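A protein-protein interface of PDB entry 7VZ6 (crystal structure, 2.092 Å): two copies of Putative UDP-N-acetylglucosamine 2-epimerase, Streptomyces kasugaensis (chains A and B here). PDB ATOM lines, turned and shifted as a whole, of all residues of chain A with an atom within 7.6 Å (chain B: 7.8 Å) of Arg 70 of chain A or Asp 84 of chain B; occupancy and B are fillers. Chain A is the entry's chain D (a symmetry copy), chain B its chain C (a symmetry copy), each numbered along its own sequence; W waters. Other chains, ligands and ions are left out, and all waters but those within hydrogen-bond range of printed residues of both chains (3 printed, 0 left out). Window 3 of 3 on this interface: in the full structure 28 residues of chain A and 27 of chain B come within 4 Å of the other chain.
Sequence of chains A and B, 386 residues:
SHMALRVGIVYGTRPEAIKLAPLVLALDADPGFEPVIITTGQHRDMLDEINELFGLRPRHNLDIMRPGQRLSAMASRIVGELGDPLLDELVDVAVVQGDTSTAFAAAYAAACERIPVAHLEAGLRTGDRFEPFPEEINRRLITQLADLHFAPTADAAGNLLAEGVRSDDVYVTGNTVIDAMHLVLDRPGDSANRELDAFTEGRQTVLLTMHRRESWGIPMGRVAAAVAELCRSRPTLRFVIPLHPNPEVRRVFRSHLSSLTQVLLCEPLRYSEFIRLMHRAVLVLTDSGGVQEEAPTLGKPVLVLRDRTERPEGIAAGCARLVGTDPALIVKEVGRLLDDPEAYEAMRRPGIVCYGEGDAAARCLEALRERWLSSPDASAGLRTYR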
ATOM      1  N   ARG A  66     -24.491  24.303 -24.356  1.00  0.00           N
ATOM      2  CA  ARG A  66     -23.716  24.532 -23.095  1.00  0.00           C
ATOM      3  C   ARG A  66     -22.215  24.566 -23.424  1.00  0.00           C
ATOM      4  O   ARG A  66     -21.832  23.880 -24.394  1.00  0.00           O
ATOM      5  CB  ARG A  66     -23.926  23.471 -21.998  1.00  0.00           C
ATOM      6  CG  ARG A  66     -25.098  22.503 -22.135  1.00  0.00           C
ATOM      7  CD  ARG A  66     -26.477  22.923 -21.657  1.00  0.00           C
ATOM      8  NE  ARG A  66     -26.546  23.590 -20.366  1.00  0.00           N
ATOM      9  CZ  ARG A  66     -27.673  23.844 -19.701  1.00  0.00           C
ATOM     10  NH1 ARG A  66     -28.850  23.484 -20.196  1.00  0.00           N
ATOM     11  NH2 ARG A  66     -27.624  24.462 -18.531  1.00  0.00           N
ATOM     12  N   GLY A  68     -20.357  22.139 -21.395  1.00  0.00           N
ATOM     13  CA  GLY A  68     -19.652  20.855 -21.542  1.00  0.00           C
ATOM     14  C   GLY A  68     -20.606  19.724 -21.911  1.00  0.00           C
ATOM     15  O   GLY A  68     -21.029  18.968 -20.993  1.00  0.00           O
ATOM     16  N   GLN A  69     -20.928  19.599 -23.208  1.00  0.00           N
ATOM     17  CA  GLN A  69     -21.946  18.647 -23.724  1.00  0.00           C
ATOM     18  C   GLN A  69     -21.392  17.932 -24.968  1.00  0.00           C
ATOM     19  O   GLN A  69     -20.673  18.544 -25.756  1.00  0.00           O
ATOM     20  CB  GLN A  69     -23.238  19.411 -24.030  1.00  0.00           C
ATOM     21  CG  GLN A  69     -23.210  19.958 -25.439  1.00  0.00           C
ATOM     22  CD  GLN A  69     -24.307  20.912 -25.821  1.00  0.00           C
ATOM     23  OE1 GLN A  69     -24.095  21.796 -26.660  1.00  0.00           O
ATOM     24  NE2 GLN A  69     -25.508  20.600 -25.368  1.00  0.00           N
ATOM     25  N   ARG A  70     -21.750  16.671 -25.124  1.00  0.00           N
ATOM     26  CA  ARG A  70     -21.373  15.827 -26.284  1.00  0.00           C
ATOM     27  C   ARG A  70     -22.052  16.389 -27.538  1.00  0.00           C
ATOM     28  O   ARG A  70     -23.208  16.873 -27.459  1.00  0.00           O
ATOM     29  CB  ARG A  70     -21.770  14.375 -26.022  1.00  0.00           C
ATOM     30  CG  ARG A  70     -20.763  13.594 -25.183  1.00  0.00           C
ATOM     31  CD  ARG A  70     -21.224  12.170 -24.927  1.00  0.00           C
ATOM     32  NE  ARG A  70     -21.323  11.322 -26.117  1.00  0.00           N
ATOM     33  CZ  ARG A  70     -21.903  10.119 -26.145  1.00  0.00           C
ATOM     34  NH1 ARG A  70     -22.453   9.614 -25.053  1.00  0.00           N
ATOM     35  NH2 ARG A  70     -21.961   9.427 -27.271  1.00  0.00           N
ATOM     36  N   LEU A  71     -21.346  16.378 -28.661  1.00  0.00           N
ATOM     37  CA  LEU A  71     -21.897  16.815 -29.967  1.00  0.00           C
ATOM     38  C   LEU A  71     -23.184  16.028 -30.274  1.00  0.00           C
ATOM     39  O   LEU A  71     -24.193  16.667 -30.589  1.00  0.00           O
ATOM     40  CB  LEU A  71     -20.842  16.593 -31.052  1.00  0.00           C
ATOM     41  CG  LEU A  71     -21.314  16.883 -32.472  1.00  0.00           C
ATOM     42  CD1 LEU A  71     -21.944  18.258 -32.557  1.00  0.00           C
ATOM     43  CD2 LEU A  71     -20.182  16.779 -33.448  1.00  0.00           C
ATOM     44  N   SER A  72     -23.152  14.706 -30.169  1.00  0.00           N
ATOM     45  CA  SER A  72     -24.296  13.808 -30.484  1.00  0.00           C
ATOM     46  C   SER A  72     -25.525  14.201 -29.653  1.00  0.00           C
ATOM     47  O   SER A  72     -26.628  14.214 -30.205  1.00  0.00           O
ATOM     48  CB  SER A  72     -23.935  12.356 -30.260  1.00  0.00           C
ATOM     49  OG  SER A  72     -23.652  12.126 -28.886  1.00  0.00           O
ATOM     50  N   ALA A  73     -25.354  14.557 -28.375  1.00  0.00           N
ATOM     51  CA  ALA A  73     -26.483  14.905 -27.487  1.00  0.00           C
ATOM     52  C   ALA A  73     -27.055  16.242 -27.954  1.00  0.00           C
ATOM     53  O   ALA A  73     -28.283  16.357 -28.069  1.00  0.00           O
ATOM     54  CB  ALA A  73     -26.057  14.947 -26.034  1.00  0.00           C
ATOM     55  N   MET A  74     -26.201  17.215 -28.258  1.00  0.00           N
ATOM     56  CA  MET A  74     -26.662  18.548 -28.720  1.00  0.00           C
ATOM     57  C   MET A  74     -27.413  18.402 -30.056  1.00  0.00           C
ATOM     58  O   MET A  74     -28.514  18.948 -30.177  1.00  0.00           O
ATOM     59  CB  MET A  74     -25.483  19.504 -28.920  1.00  0.00           C
ATOM     60  CG  MET A  74     -25.930  20.942 -29.125  1.00  0.00           C
ATOM     61  SD  MET A  74     -24.920  21.833 -30.372  1.00  0.00           S
ATOM     62  CE  MET A  74     -23.244  21.510 -29.814  1.00  0.00           C
ATOM     63  N   ALA A  75     -26.812  17.721 -31.042  1.00  0.00           N
ATOM     64  CA  ALA A  75     -27.415  17.541 -32.381  1.00  0.00           C
ATOM     65  C   ALA A  75     -28.753  16.773 -32.232  1.00  0.00           C
ATOM     66  O   ALA A  75     -29.755  17.184 -32.828  1.00  0.00           O
ATOM     67  CB  ALA A  75     -26.450  16.856 -33.290  1.00  0.00           C
ATOM     68  N   SER A  76     -28.780  15.730 -31.406  1.00  0.00           N
ATOM     69  CA  SER A  76     -30.002  14.947 -31.097  1.00  0.00           C
ATOM     70  C   SER A  76     -31.112  15.893 -30.620  1.00  0.00           C
ATOM     71  O   SER A  76     -32.257  15.805 -31.132  1.00  0.00           O
ATOM     72  CB  SER A  76     -29.744  13.872 -30.092  1.00  0.00           C
ATOM     73  OG  SER A  76     -30.968  13.281 -29.692  1.00  0.00           O
ATOM     74  N   ILE B  38     -25.345  -3.803 -35.036  1.00  0.00           N
ATOM     75  CA  ILE B  38     -26.317  -3.022 -34.228  1.00  0.00           C
ATOM     76  C   ILE B  38     -27.525  -2.757 -35.115  1.00  0.00           C
ATOM     77  O   ILE B  38     -27.335  -2.126 -36.174  1.00  0.00           O
ATOM     78  CB  ILE B  38     -25.689  -1.716 -33.691  1.00  0.00           C
ATOM     79  CG1 ILE B  38     -24.446  -1.998 -32.861  1.00  0.00           C
ATOM     80  CG2 ILE B  38     -26.708  -0.936 -32.889  1.00  0.00           C
ATOM     81  CD1 ILE B  38     -23.565  -0.798 -32.652  1.00  0.00           C
ATOM     82  N   HIS B  60     -26.493  -5.723 -30.409  1.00  0.00           N
ATOM     83  CA  HIS B  60     -27.462  -4.769 -29.815  1.00  0.00           C
ATOM     84  C   HIS B  60     -28.600  -4.517 -30.794  1.00  0.00           C
ATOM     85  O   HIS B  60     -28.329  -4.346 -32.006  1.00  0.00           O
ATOM     86  CB  HIS B  60     -26.784  -3.445 -29.442  1.00  0.00           C
ATOM     87  CG  HIS B  60     -25.765  -3.555 -28.366  1.00  0.00           C
ATOM     88  ND1 HIS B  60     -26.071  -3.403 -27.026  1.00  0.00           N
ATOM     89  CD2 HIS B  60     -24.436  -3.780 -28.432  1.00  0.00           C
ATOM     90  CE1 HIS B  60     -24.963  -3.551 -26.314  1.00  0.00           C
ATOM     91  NE2 HIS B  60     -23.939  -3.790 -27.160  1.00  0.00           N
ATOM     92  N   LEU B  62     -31.437  -1.639 -30.843  1.00  0.00           N
ATOM     93  CA  LEU B  62     -32.044  -0.388 -30.330  1.00  0.00           C
ATOM     94  C   LEU B  62     -33.495  -0.484 -30.792  1.00  0.00           C
ATOM     95  O   LEU B  62     -33.696  -0.816 -31.964  1.00  0.00           O
ATOM     96  CB  LEU B  62     -31.346   0.827 -30.934  1.00  0.00           C
ATOM     97  CG  LEU B  62     -29.826   0.851 -30.815  1.00  0.00           C
ATOM     98  CD1 LEU B  62     -29.289   2.212 -31.193  1.00  0.00           C
ATOM     99  CD2 LEU B  62     -29.389   0.483 -29.405  1.00  0.00           C
ATOM    100  N   ILE B  78     -31.656   8.043 -33.020  1.00  0.00           N
ATOM    101  CA  ILE B  78     -30.467   7.290 -33.519  1.00  0.00           C
ATOM    102  C   ILE B  78     -29.215   8.135 -33.248  1.00  0.00           C
ATOM    103  O   ILE B  78     -28.238   7.608 -32.703  1.00  0.00           O
ATOM    104  CB  ILE B  78     -30.618   6.887 -34.998  1.00  0.00           C
ATOM    105  CG1 ILE B  78     -31.761   5.872 -35.168  1.00  0.00           C
ATOM    106  CG2 ILE B  78     -29.308   6.338 -35.519  1.00  0.00           C
ATOM    107  CD1 ILE B  78     -32.104   5.560 -36.608  1.00  0.00           C
ATOM    108  N   VAL B  79     -29.259   9.427 -33.575  1.00  0.00           N
ATOM    109  CA  VAL B  79     -28.112  10.355 -33.329  1.00  0.00           C
ATOM    110  C   VAL B  79     -27.776  10.334 -31.832  1.00  0.00           C
ATOM    111  O   VAL B  79     -26.572  10.291 -31.496  1.00  0.00           O
ATOM    112  CB  VAL B  79     -28.412  11.780 -33.820  1.00  0.00           C
ATOM    113  CG1 VAL B  79     -27.314  12.758 -33.406  1.00  0.00           C
ATOM    114  CG2 VAL B  79     -28.616  11.804 -35.327  1.00  0.00           C
ATOM    115  N   GLY B  80     -28.798  10.320 -30.981  1.00  0.00           N
ATOM    116  CA  GLY B  80     -28.651  10.428 -29.519  1.00  0.00           C
ATOM    117  C   GLY B  80     -28.133   9.165 -28.876  1.00  0.00           C
ATOM    118  O   GLY B  80     -27.347   9.276 -27.903  1.00  0.00           O
ATOM    119  N   GLU B  81     -28.508   7.993 -29.395  1.00  0.00           N
ATOM    120  CA  GLU B  81     -28.393   6.711 -28.650  1.00  0.00           C
ATOM    121  C   GLU B  81     -27.426   5.729 -29.310  1.00  0.00           C
ATOM    122  O   GLU B  81     -27.014   4.832 -28.597  1.00  0.00           O
ATOM    123  CB  GLU B  81     -29.771   6.069 -28.495  1.00  0.00           C
ATOM    124  CG  GLU B  81     -30.758   6.976 -27.783  1.00  0.00           C
ATOM    125  CD  GLU B  81     -32.180   6.448 -27.724  1.00  0.00           C
ATOM    126  OE1 GLU B  81     -32.347   5.225 -27.811  1.00  0.00           O
ATOM    127  OE2 GLU B  81     -33.118   7.271 -27.631  1.00  0.00           O
ATOM    128  N   LEU B  82     -27.050   5.887 -30.589  1.00  0.00           N
ATOM    129  CA  LEU B  82     -26.208   4.864 -31.259  1.00  0.00           C
ATOM    130  C   LEU B  82     -24.755   4.965 -30.785  1.00  0.00           C
ATOM    131  O   LEU B  82     -24.056   3.938 -30.816  1.00  0.00           O
ATOM    132  CB  LEU B  82     -26.275   5.011 -32.781  1.00  0.00           C
ATOM    133  CG  LEU B  82     -25.546   3.904 -33.539  1.00  0.00           C
ATOM    134  CD1 LEU B  82     -26.266   2.576 -33.355  1.00  0.00           C
ATOM    135  CD2 LEU B  82     -25.410   4.238 -35.008  1.00  0.00           C
ATOM    136  N   GLY B  83     -24.307   6.151 -30.377  1.00  0.00           N
ATOM    137  CA  GLY B  83     -22.914   6.356 -29.942  1.00  0.00           C
ATOM    138  C   GLY B  83     -22.498   5.395 -28.836  1.00  0.00           C
ATOM    139  O   GLY B  83     -21.377   4.883 -28.908  1.00  0.00           O
ATOM    140  N   ASP B  84     -23.369   5.138 -27.853  1.00  0.00           N
ATOM    141  CA  ASP B  84     -23.001   4.342 -26.646  1.00  0.00           C
ATOM    142  C   ASP B  84     -22.673   2.903 -27.031  1.00  0.00           C
ATOM    143  O   ASP B  84     -21.573   2.453 -26.740  1.00  0.00           O
ATOM    144  CB  ASP B  84     -24.042   4.491 -25.540  1.00  0.00           C
ATOM    145  CG  ASP B  84     -23.910   5.840 -24.826  1.00  0.00           C
ATOM    146  OD1 ASP B  84     -22.745   6.377 -24.706  1.00  0.00           O
ATOM    147  OD2 ASP B  84     -24.966   6.378 -24.440  1.00  0.00           O
ATOM    148  N   PRO B  85     -23.557   2.144 -27.723  1.00  0.00           N
ATOM    149  CA  PRO B  85     -23.182   0.816 -28.203  1.00  0.00           C
ATOM    150  C   PRO B  85     -21.960   0.809 -29.133  1.00  0.00           C
ATOM    151  O   PRO B  85     -21.208  -0.106 -29.020  1.00  0.00           O
ATOM    152  CB  PRO B  85     -24.435   0.270 -28.893  1.00  0.00           C
ATOM    153  CG  PRO B  85     -25.387   1.422 -29.013  1.00  0.00           C
ATOM    154  CD  PRO B  85     -24.957   2.466 -28.002  1.00  0.00           C
ATOM    155  N   LEU B  86     -21.749   1.825 -29.981  1.00  0.00           N
ATOM    156  CA  LEU B  86     -20.554   1.873 -30.870  1.00  0.00           C
ATOM    157  C   LEU B  86     -19.293   1.945 -29.993  1.00  0.00           C
ATOM    158  O   LEU B  86     -18.294   1.272 -30.311  1.00  0.00           O
ATOM    159  CB  LEU B  86     -20.620   3.090 -31.812  1.00  0.00           C
ATOM    160  CG  LEU B  86     -21.596   2.997 -32.990  1.00  0.00           C
ATOM    161  CD1 LEU B  86     -21.623   4.322 -33.750  1.00  0.00           C
ATOM    162  CD2 LEU B  86     -21.225   1.857 -33.925  1.00  0.00           C
ATOM    163  N   LEU B  87     -19.323   2.770 -28.940  1.00  0.00           N
ATOM    164  CA  LEU B  87     -18.182   2.937 -27.998  1.00  0.00           C
ATOM    165  C   LEU B  87     -18.030   1.675 -27.136  1.00  0.00           C
ATOM    166  O   LEU B  87     -16.908   1.139 -27.090  1.00  0.00           O
ATOM    167  CB  LEU B  87     -18.406   4.199 -27.152  1.00  0.00           C
ATOM    168  CG  LEU B  87     -18.347   5.516 -27.920  1.00  0.00           C
ATOM    169  CD1 LEU B  87     -18.719   6.687 -27.025  1.00  0.00           C
ATOM    170  CD2 LEU B  87     -16.965   5.717 -28.511  1.00  0.00           C
ATOM    171  N   ASP B  88     -19.120   1.174 -26.552  1.00  0.00           N
ATOM    172  CA  ASP B  88     -19.128  -0.051 -25.698  1.00  0.00           C
ATOM    173  C   ASP B  88     -18.552  -1.247 -26.470  1.00  0.00           C
ATOM    174  O   ASP B  88     -17.810  -2.032 -25.858  1.00  0.00           O
ATOM    175  CB  ASP B  88     -20.536  -0.375 -25.187  1.00  0.00           C
ATOM    176  CG  ASP B  88     -21.021   0.599 -24.124  1.00  0.00           C
ATOM    177  OD1 ASP B  88     -20.160   1.292 -23.526  1.00  0.00           O
ATOM    178  OD2 ASP B  88     -22.254   0.689 -23.912  1.00  0.00           O
ATOM    179  N   GLU B  89     -18.859  -1.378 -27.766  1.00  0.00           N
ATOM    180  CA  GLU B  89     -18.411  -2.527 -28.599  1.00  0.00           C
ATOM    181  C   GLU B  89     -17.047  -2.257 -29.226  1.00  0.00           C
ATOM    182  O   GLU B  89     -16.575  -3.115 -29.982  1.00  0.00           O
ATOM    183  CB  GLU B  89     -19.478  -2.823 -29.649  1.00  0.00           C
ATOM    184  CG  GLU B  89     -20.750  -3.361 -29.060  1.00  0.00           C
ATOM    185  CD  GLU B  89     -20.561  -4.658 -28.281  1.00  0.00           C
ATOM    186  OE1 GLU B  89     -19.680  -5.455 -28.690  1.00  0.00           O
ATOM    187  OE2 GLU B  89     -21.270  -4.837 -27.252  1.00  0.00           O
ATOM    188  N   LEU B  90     -16.421  -1.117 -28.929  1.00  0.00           N
ATOM    189  CA  LEU B  90     -15.041  -0.812 -29.377  1.00  0.00           C
ATOM    190  C   LEU B  90     -14.992  -0.880 -30.903  1.00  0.00           C
ATOM    191  O   LEU B  90     -14.046  -1.434 -31.478  1.00  0.00           O
ATOM    192  CB  LEU B  90     -14.089  -1.814 -28.713  1.00  0.00           C
ATOM    193  CG  LEU B  90     -12.589  -1.522 -28.860  1.00  0.00           C
ATOM    194  CD1 LEU B  90     -12.224  -0.182 -28.207  1.00  0.00           C
ATOM    195  CD2 LEU B  90     -11.744  -2.666 -28.288  1.00  0.00           C
ATOM    196  N   ALA B 109     -23.883   9.666 -36.216  1.00  0.00           N
ATOM    197  CA  ALA B 109     -23.571   9.254 -34.834  1.00  0.00           C
ATOM    198  C   ALA B 109     -22.128   8.724 -34.790  1.00  0.00           C
ATOM    199  O   ALA B 109     -21.381   9.110 -33.856  1.00  0.00           O
ATOM    200  CB  ALA B 109     -24.579   8.248 -34.350  1.00  0.00           C
ATOM    201  N   CYS B 112     -19.635  11.611 -35.065  1.00  0.00           N
ATOM    202  CA  CYS B 112     -19.599  12.367 -33.786  1.00  0.00           C
ATOM    203  C   CYS B 112     -18.567  11.744 -32.829  1.00  0.00           C
ATOM    204  O   CYS B 112     -17.967  12.503 -32.057  1.00  0.00           O
ATOM    205  CB  CYS B 112     -20.960  12.406 -33.121  1.00  0.00           C
ATOM    206  SG  CYS B 112     -22.084  13.568 -33.926  1.00  0.00           S
ATOM    207  N   GLU B 113     -18.337  10.427 -32.926  1.00  0.00           N
ATOM    208  CA  GLU B 113     -17.367   9.676 -32.098  1.00  0.00           C
ATOM    209  C   GLU B 113     -16.043   9.512 -32.848  1.00  0.00           C
ATOM    210  O   GLU B 113     -15.180   8.748 -32.362  1.00  0.00           O
ATOM    211  CB  GLU B 113     -17.960   8.320 -31.716  1.00  0.00           C
ATOM    212  CG  GLU B 113     -19.259   8.383 -30.930  1.00  0.00           C
ATOM    213  CD  GLU B 113     -19.293   9.364 -29.761  1.00  0.00           C
ATOM    214  OE1 GLU B 113     -18.230   9.598 -29.163  1.00  0.00           O
ATOM    215  OE2 GLU B 113     -20.388   9.927 -29.476  1.00  0.00           O
HETATM  216  O   HOH W   1     -25.755  11.520 -27.290  1.00  0.00           O
HETATM  217  O   HOH W   2     -18.560  11.387 -27.143  1.00  0.00           O
HETATM  218  O   HOH W   3     -20.793  13.148 -29.547  1.00  0.00           O
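The side-chain carboxylate (OD1) of Asp 84 of chain B lies within salt-bridge range of the guanidinium group (NH1) of Arg 70 of chain A.
NH2 of Arg 70 of chain A lies within salt-bridge range of OE2 of Glu 113 of chain B (2.8 Å).
SG of Cys 112 of chain B touches CG of Leu 71 of chain A (3.7 Å).
O of Val 79 of chain B touches CB of Ser 72 of chain A, 3.6 Å away.
Glu 113 of chain B touches Ser 72 of chain A (OE2 to OG, 3.98 Å).
Ser 76 of chain A touches Val 79 of chain B (N to CG1, 3.9 Å).
Ser 76 of chain A touches Gly 80 of chain B (CB to CA, 3.7 Å).
Arg 70 of chain A touches just these residues of chain B: Asp 84 (3.3 Å) and Glu 113 (2.8 Å).
Of chain A, only Arg 70 comes within 4 Å of Asp 84 of chain B.
Printed residues of chain B within 4 Å of Leu 71 of chain A: Cys 112 (3.7 Å).
Printed residues of chain A within 4 Å of Glu 113 of chain B: Arg 70 (2.8 Å) and Ser 72 (3.98 Å).
Printed residues of chain B within 4 Å of Ser 72 of chain A: Val 79 (3.6 Å) and Glu 113 (3.98 Å).
Of the printed residues of chain B, Ser 76 of chain A touches Val 79 (3.9 Å) and Gly 80 (3.7 Å).
Of the printed residues of chain A, Val 79 of chain B touches Ser 72 and Ser 76.
Gly 68 of chain A touches none of the printed residues of chain B.
Arg 66 of chain A touches none of the printed residues of chain B.
The nearest printed residue of chain A that does not touch Gly 80 of chain B is Ser 72 of chain A (4.3 Å).
Of the 10 printed residues of chain A, 4 touch a printed residue of chain B.
Hydrophobic or aromatic side chains of chain A that line the printed part of chain B: Leu 71.
Among the printed residues, Asp or Glu carboxylates within 4 Å of a Lys or Arg side-chain nitrogen of the other chain: Arg 70 of chain A with Asp 84 of chain B and Arg 70 of chain A with Glu 113 of chain B.
No position is printed for both chains.
Water W1 lies within hydrogen-bond range of the side-chain hydroxyl (OG) of Ser 72 of chain A (2.7 Å), the backbone carbonyl oxygen (O) of Gly 80 of chain B (2.8 Å) and the backbone NH (N) of Ala 73 of chain A (3.2 Å).
Water W2 lies within hydrogen-bond range of OE1 of Glu 113 of chain B and NE of Arg 70 of chain A.
Water W3 lies within hydrogen-bond range of the backbone NH (N) of Ser 72 of chain A (2.9 Å), the side-chain carboxylate (OE2) of Glu 113 of chain B (3.2 Å) and the backbone NH (N) of Leu 71 of chain A (3.4 Å).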
